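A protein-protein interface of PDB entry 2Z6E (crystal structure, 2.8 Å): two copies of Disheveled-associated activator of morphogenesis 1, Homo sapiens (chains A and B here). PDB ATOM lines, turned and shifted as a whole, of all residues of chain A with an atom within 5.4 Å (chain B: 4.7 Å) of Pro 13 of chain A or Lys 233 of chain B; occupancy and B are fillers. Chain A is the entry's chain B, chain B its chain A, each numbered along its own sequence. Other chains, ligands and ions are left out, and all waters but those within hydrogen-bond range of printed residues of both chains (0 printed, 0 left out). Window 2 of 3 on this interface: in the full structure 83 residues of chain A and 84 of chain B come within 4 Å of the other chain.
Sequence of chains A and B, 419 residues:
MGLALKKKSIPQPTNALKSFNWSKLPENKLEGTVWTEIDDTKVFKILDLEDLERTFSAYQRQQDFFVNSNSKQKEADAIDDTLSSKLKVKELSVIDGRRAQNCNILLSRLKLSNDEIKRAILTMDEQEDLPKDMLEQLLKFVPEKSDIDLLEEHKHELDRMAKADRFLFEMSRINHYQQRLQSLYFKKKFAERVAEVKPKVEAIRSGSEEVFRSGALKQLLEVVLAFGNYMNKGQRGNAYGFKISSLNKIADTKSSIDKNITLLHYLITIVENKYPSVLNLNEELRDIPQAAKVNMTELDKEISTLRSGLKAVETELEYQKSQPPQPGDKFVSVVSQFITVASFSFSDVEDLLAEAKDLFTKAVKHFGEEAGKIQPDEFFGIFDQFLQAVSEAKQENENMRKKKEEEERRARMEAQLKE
The side-chain hydroxyl (OH) of Tyr 230 of chain B is in hydrogen-bond range of the side-chain carboxylate (OE2) of Glu 53 of chain A.
The side-chain hydroxyl (OG1) of Thr 14 of chain A sits at hydrogen-bond distance from the side-chain carboxylate (OE1) of Glu 53 of chain A.
O of Pro 11 of chain A touches CD1 of Tyr 230 of chain B (3.0 Å). Tyr 230 of chain B touches Gln 12 of chain A. Gln 12 of chain A touches Lys 233 of chain B (NE2 to CD, 3.5 Å). Pro 13 of chain A touches Tyr 230 of chain B. Pro 13 of chain A touches Lys 233 of chain B. CD1 of Leu 17 of chain A touches CD2 of Tyr 230 of chain B (3.6 Å). CD1 of Leu 150 of chain A touches CB of Asn 232 of chain B, 3.7 Å away. O of Lys 233 of chain B touches CD2 of Leu 150 of chain A, 3.8 Å away. CD1 of Leu 150 of chain A touches CG of Arg 236 of chain B (3.7 Å).
Printed residues of chain B within 4 Å of Gln 12 of chain A: Tyr 230 (3.8 Å) and Lys 233 (3.5 Å). Of the printed residues of chain B, Pro 13 of chain A touches Tyr 230 (3.3 Å) and Lys 233 (3.8 Å). Asn 15 of chain A touches none of the printed residues of chain B. Printed residues of chain B within 4 Å of Leu 150 of chain A: Asn 232 (3.7 Å), Lys 233 (3.8 Å) and Arg 236 (3.7 Å). Printed residues of chain A within 4 Å of Tyr 230 of chain B: Pro 11 (3.0 Å), Gln 12 (3.8 Å), Pro 13 (3.3 Å), Leu 17 (3.6 Å) and Glu 53 (2.6 Å). Of the printed residues of chain A, Asn 232 of chain B touches Leu 150. Of chain A, only Gln 12, Pro 13 and Leu 150 come within 4 Å of Lys 233 of chain B. Gly 234 of chain B touches none of the printed residues of chain A. The nearest residue of chain B that does not touch Pro 13 of chain A is Met 231 of chain B (4.6 Å). The nearest residue of chain A that does not touch Lys 233 of chain B is Glu 153 of chain A (5.1 Å). The nearest printed residue of chain A that does not touch Arg 236 of chain B is Glu 153 of chain A (7.3 Å).
Hydrophobic or aromatic side chains of chain B that line the printed part of chain A: Tyr 230. Of the 9 printed residues of chain A, 6 touch a printed residue of chain B. Printed residues of chain A that touch a printed residue of chain B: Pro 11, Gln 12, Pro 13, Leu 17, Glu 53 and Leu 150. Among the printed residues, 10 pairs touch across the chains. Among the printed residues, no Asp or Glu carboxylate lies within 4 Å of a Lys or Arg side-chain nitrogen of the other chain.
No position is printed for both chains. Of the 10 pairs that touch across the chains among the printed residues, none has its exchanged pair printed and touching as well.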
ATOM      1  N   PRO A  11      19.760   1.169  -5.112  1.00  0.00           N
ATOM      2  CA  PRO A  11      20.766   0.867  -6.132  1.00  0.00           C
ATOM      3  C   PRO A  11      20.504   1.805  -7.302  1.00  0.00           C
ATOM      4  O   PRO A  11      19.449   1.736  -7.919  1.00  0.00           O
ATOM      5  CB  PRO A  11      20.479  -0.587  -6.479  1.00  0.00           C
ATOM      6  CG  PRO A  11      19.020  -0.686  -6.281  1.00  0.00           C
ATOM      7  CD  PRO A  11      18.802   0.061  -4.981  1.00  0.00           C
ATOM      8  N   GLN A  12      21.438   2.701  -7.598  1.00  0.00           N
ATOM      9  CA  GLN A  12      21.218   3.616  -8.705  1.00  0.00           C
ATOM     10  C   GLN A  12      22.139   3.352  -9.890  1.00  0.00           C
ATOM     11  O   GLN A  12      23.262   2.869  -9.728  1.00  0.00           O
ATOM     12  CB  GLN A  12      21.323   5.069  -8.225  1.00  0.00           C
ATOM     13  CG  GLN A  12      20.271   5.418  -7.160  1.00  0.00           C
ATOM     14  CD  GLN A  12      20.167   6.910  -6.861  1.00  0.00           C
ATOM     15  OE1 GLN A  12      19.692   7.311  -5.787  1.00  0.00           O
ATOM     16  NE2 GLN A  12      20.599   7.742  -7.814  1.00  0.00           N
ATOM     17  N   PRO A  13      21.656   3.657 -11.106  1.00  0.00           N
ATOM     18  CA  PRO A  13      22.361   3.481 -12.379  1.00  0.00           C
ATOM     19  C   PRO A  13      23.727   4.143 -12.517  1.00  0.00           C
ATOM     20  O   PRO A  13      23.906   5.322 -12.208  1.00  0.00           O
ATOM     21  CB  PRO A  13      21.361   4.012 -13.405  1.00  0.00           C
ATOM     22  CG  PRO A  13      20.599   5.034 -12.634  1.00  0.00           C
ATOM     23  CD  PRO A  13      20.359   4.316 -11.333  1.00  0.00           C
ATOM     24  N   THR A  14      24.687   3.364 -12.997  1.00  0.00           N
ATOM     25  CA  THR A  14      26.039   3.855 -13.199  1.00  0.00           C
ATOM     26  C   THR A  14      26.040   4.884 -14.314  1.00  0.00           C
ATOM     27  O   THR A  14      26.850   5.810 -14.313  1.00  0.00           O
ATOM     28  CB  THR A  14      26.994   2.711 -13.569  1.00  0.00           C
ATOM     29  OG1 THR A  14      26.335   1.802 -14.470  1.00  0.00           O
ATOM     30  CG2 THR A  14      27.430   1.971 -12.316  1.00  0.00           C
ATOM     31  N   ASN A  15      25.126   4.715 -15.262  1.00  0.00           N
ATOM     32  CA  ASN A  15      25.009   5.640 -16.388  1.00  0.00           C
ATOM     33  C   ASN A  15      23.635   6.306 -16.419  1.00  0.00           C
ATOM     34  O   ASN A  15      22.712   5.904 -15.708  1.00  0.00           O
ATOM     35  CB  ASN A  15      25.247   4.903 -17.713  1.00  0.00           C
ATOM     36  CG  ASN A  15      26.719   4.633 -17.987  1.00  0.00           C
ATOM     37  OD1 ASN A  15      27.480   5.537 -18.350  1.00  0.00           O
ATOM     38  ND2 ASN A  15      27.123   3.383 -17.814  1.00  0.00           N
ATOM     39  N   LEU A  17      19.959   7.311 -17.709  1.00  0.00           N
ATOM     40  CA  LEU A  17      18.844   6.578 -18.320  1.00  0.00           C
ATOM     41  C   LEU A  17      17.779   7.559 -18.766  1.00  0.00           C
ATOM     42  O   LEU A  17      17.885   8.747 -18.496  1.00  0.00           O
ATOM     43  CB  LEU A  17      18.213   5.621 -17.310  1.00  0.00           C
ATOM     44  CG  LEU A  17      19.056   4.464 -16.799  1.00  0.00           C
ATOM     45  CD1 LEU A  17      18.317   3.758 -15.690  1.00  0.00           C
ATOM     46  CD2 LEU A  17      19.355   3.520 -17.939  1.00  0.00           C
ATOM     47  N   GLU A  53      19.273  -0.790 -17.963  1.00  0.00           N
ATOM     48  CA  GLU A  53      20.162   0.299 -18.338  1.00  0.00           C
ATOM     49  C   GLU A  53      20.494   0.363 -19.816  1.00  0.00           C
ATOM     50  O   GLU A  53      20.412   1.437 -20.413  1.00  0.00           O
ATOM     51  CB  GLU A  53      21.457   0.242 -17.526  1.00  0.00           C
ATOM     52  CG  GLU A  53      21.275   0.469 -16.026  1.00  0.00           C
ATOM     53  CD  GLU A  53      22.604   0.697 -15.313  1.00  0.00           C
ATOM     54  OE1 GLU A  53      23.233   1.761 -15.534  1.00  0.00           O
ATOM     55  OE2 GLU A  53      23.032  -0.189 -14.541  1.00  0.00           O
ATOM     56  N   LEU A 150      16.139  16.932 -13.413  1.00  0.00           N
ATOM     57  CA  LEU A 150      16.613  15.844 -14.263  1.00  0.00           C
ATOM     58  C   LEU A 150      17.597  16.309 -15.308  1.00  0.00           C
ATOM     59  O   LEU A 150      18.484  15.563 -15.684  1.00  0.00           O
ATOM     60  CB  LEU A 150      15.444  15.132 -14.950  1.00  0.00           C
ATOM     61  CG  LEU A 150      14.973  13.878 -14.201  1.00  0.00           C
ATOM     62  CD1 LEU A 150      13.570  13.458 -14.638  1.00  0.00           C
ATOM     63  CD2 LEU A 150      15.988  12.769 -14.436  1.00  0.00           C
ATOM     64  N   GLU A 153      21.919  17.369 -14.131  1.00  0.00           N
ATOM     65  CA  GLU A 153      23.052  16.458 -14.228  1.00  0.00           C
ATOM     66  C   GLU A 153      23.717  16.431 -15.588  1.00  0.00           C
ATOM     67  O   GLU A 153      24.542  15.553 -15.838  1.00  0.00           O
ATOM     68  CB  GLU A 153      22.646  15.022 -13.894  1.00  0.00           C
ATOM     69  CG  GLU A 153      22.111  14.805 -12.506  1.00  0.00           C
ATOM     70  CD  GLU A 153      20.767  15.461 -12.318  1.00  0.00           C
ATOM     71  OE1 GLU A 153      19.953  15.391 -13.264  1.00  0.00           O
ATOM     72  OE2 GLU A 153      20.519  16.036 -11.233  1.00  0.00           O
ATOM     73  N   ASN B 229      12.166   4.691  -9.526  1.00  0.00           N
ATOM     74  CA  ASN B 229      13.258   5.034  -8.627  1.00  0.00           C
ATOM     75  C   ASN B 229      14.618   4.796  -9.283  1.00  0.00           C
ATOM     76  O   ASN B 229      15.547   5.572  -9.084  1.00  0.00           O
ATOM     77  CB  ASN B 229      13.146   4.253  -7.314  1.00  0.00           C
ATOM     78  CG  ASN B 229      12.089   4.840  -6.370  1.00  0.00           C
ATOM     79  OD1 ASN B 229      11.277   5.680  -6.762  1.00  0.00           O
ATOM     80  ND2 ASN B 229      12.099   4.393  -5.125  1.00  0.00           N
ATOM     81  N   TYR B 230      14.738   3.746 -10.087  1.00  0.00           N
ATOM     82  CA  TYR B 230      16.006   3.470 -10.756  1.00  0.00           C
ATOM     83  C   TYR B 230      16.183   4.430 -11.921  1.00  0.00           C
ATOM     84  O   TYR B 230      17.235   5.046 -12.085  1.00  0.00           O
ATOM     85  CB  TYR B 230      16.041   2.038 -11.294  1.00  0.00           C
ATOM     86  CG  TYR B 230      17.430   1.545 -11.686  1.00  0.00           C
ATOM     87  CD1 TYR B 230      18.382   1.249 -10.712  1.00  0.00           C
ATOM     88  CD2 TYR B 230      17.788   1.369 -13.026  1.00  0.00           C
ATOM     89  CE1 TYR B 230      19.649   0.789 -11.052  1.00  0.00           C
ATOM     90  CE2 TYR B 230      19.061   0.911 -13.378  1.00  0.00           C
ATOM     91  CZ  TYR B 230      19.983   0.623 -12.381  1.00  0.00           C
ATOM     92  OH  TYR B 230      21.245   0.173 -12.697  1.00  0.00           O
ATOM     93  N   MET B 231      15.131   4.548 -12.721  1.00  0.00           N
ATOM     94  CA  MET B 231      15.132   5.405 -13.898  1.00  0.00           C
ATOM     95  C   MET B 231      15.444   6.868 -13.581  1.00  0.00           C
ATOM     96  O   MET B 231      16.595   7.215 -13.327  1.00  0.00           O
ATOM     97  CB  MET B 231      13.780   5.291 -14.595  1.00  0.00           C
ATOM     98  CG  MET B 231      13.398   3.877 -14.967  1.00  0.00           C
ATOM     99  SD  MET B 231      13.556   3.550 -16.716  1.00  0.00           S
ATOM    100  CE  MET B 231      12.569   2.122 -16.833  1.00  0.00           C
ATOM    101  N   ASN B 232      14.436   7.734 -13.605  1.00  0.00           N
ATOM    102  CA  ASN B 232      14.690   9.131 -13.311  1.00  0.00           C
ATOM    103  C   ASN B 232      15.263   9.311 -11.902  1.00  0.00           C
ATOM    104  O   ASN B 232      14.533   9.441 -10.921  1.00  0.00           O
ATOM    105  CB  ASN B 232      13.424   9.982 -13.534  1.00  0.00           C
ATOM    106  CG  ASN B 232      12.147   9.316 -13.040  1.00  0.00           C
ATOM    107  OD1 ASN B 232      11.117   9.371 -13.717  1.00  0.00           O
ATOM    108  ND2 ASN B 232      12.195   8.712 -11.857  1.00  0.00           N
ATOM    109  N   LYS B 233      16.593   9.300 -11.824  1.00  0.00           N
ATOM    110  CA  LYS B 233      17.297   9.459 -10.558  1.00  0.00           C
ATOM    111  C   LYS B 233      17.467  10.938 -10.188  1.00  0.00           C
ATOM    112  O   LYS B 233      17.021  11.838 -10.911  1.00  0.00           O
ATOM    113  CB  LYS B 233      18.674   8.767 -10.613  1.00  0.00           C
ATOM    114  CG  LYS B 233      19.795   9.582 -11.268  1.00  0.00           C
ATOM    115  CD  LYS B 233      21.155   8.896 -11.087  1.00  0.00           C
ATOM    116  CE  LYS B 233      22.313   9.775 -11.580  1.00  0.00           C
ATOM    117  NZ  LYS B 233      23.634   9.055 -11.611  1.00  0.00           N
ATOM    118  N   GLY B 234      18.121  11.178  -9.058  1.00  0.00           N
ATOM    119  CA  GLY B 234      18.315  12.536  -8.591  1.00  0.00           C
ATOM    120  C   GLY B 234      17.349  12.809  -7.452  1.00  0.00           C
ATOM    121  O   GLY B 234      17.208  11.997  -6.533  1.00  0.00           O
ATOM    122  N   GLN B 235      16.677  13.953  -7.517  1.00  0.00           N
ATOM    123  CA  GLN B 235      15.718  14.358  -6.497  1.00  0.00           C
ATOM    124  C   GLN B 235      14.337  14.012  -7.022  1.00  0.00           C
ATOM    125  O   GLN B 235      13.335  14.203  -6.334  1.00  0.00           O
ATOM    126  CB  GLN B 235      15.853  15.862  -6.269  1.00  0.00           C
ATOM    127  CG  GLN B 235      14.834  16.510  -5.360  1.00  0.00           C
ATOM    128  CD  GLN B 235      15.012  18.030  -5.307  1.00  0.00           C
ATOM    129  OE1 GLN B 235      14.214  18.738  -4.694  1.00  0.00           O
ATOM    130  NE2 GLN B 235      16.067  18.533  -5.952  1.00  0.00           N
ATOM    131  N   ARG B 236      14.311  13.495  -8.252  1.00  0.00           N
ATOM    132  CA  ARG B 236      13.076  13.099  -8.927  1.00  0.00           C
ATOM    133  C   ARG B 236      12.636  11.687  -8.527  1.00  0.00           C
ATOM    134  O   ARG B 236      11.596  11.196  -8.970  1.00  0.00           O
ATOM    135  CB  ARG B 236      13.276  13.162 -10.443  1.00  0.00           C
ATOM    136  CG  ARG B 236      12.398  14.171 -11.179  1.00  0.00           C
ATOM    137  CD  ARG B 236      10.947  13.698 -11.385  1.00  0.00           C
ATOM    138  NE  ARG B 236      10.042  13.984 -10.262  1.00  0.00           N
ATOM    139  CZ  ARG B 236       8.721  14.138 -10.392  1.00  0.00           C
ATOM    140  NH1 ARG B 236       8.160  14.037 -11.594  1.00  0.00           N
ATOM    141  NH2 ARG B 236       7.956  14.389  -9.332  1.00  0.00           N
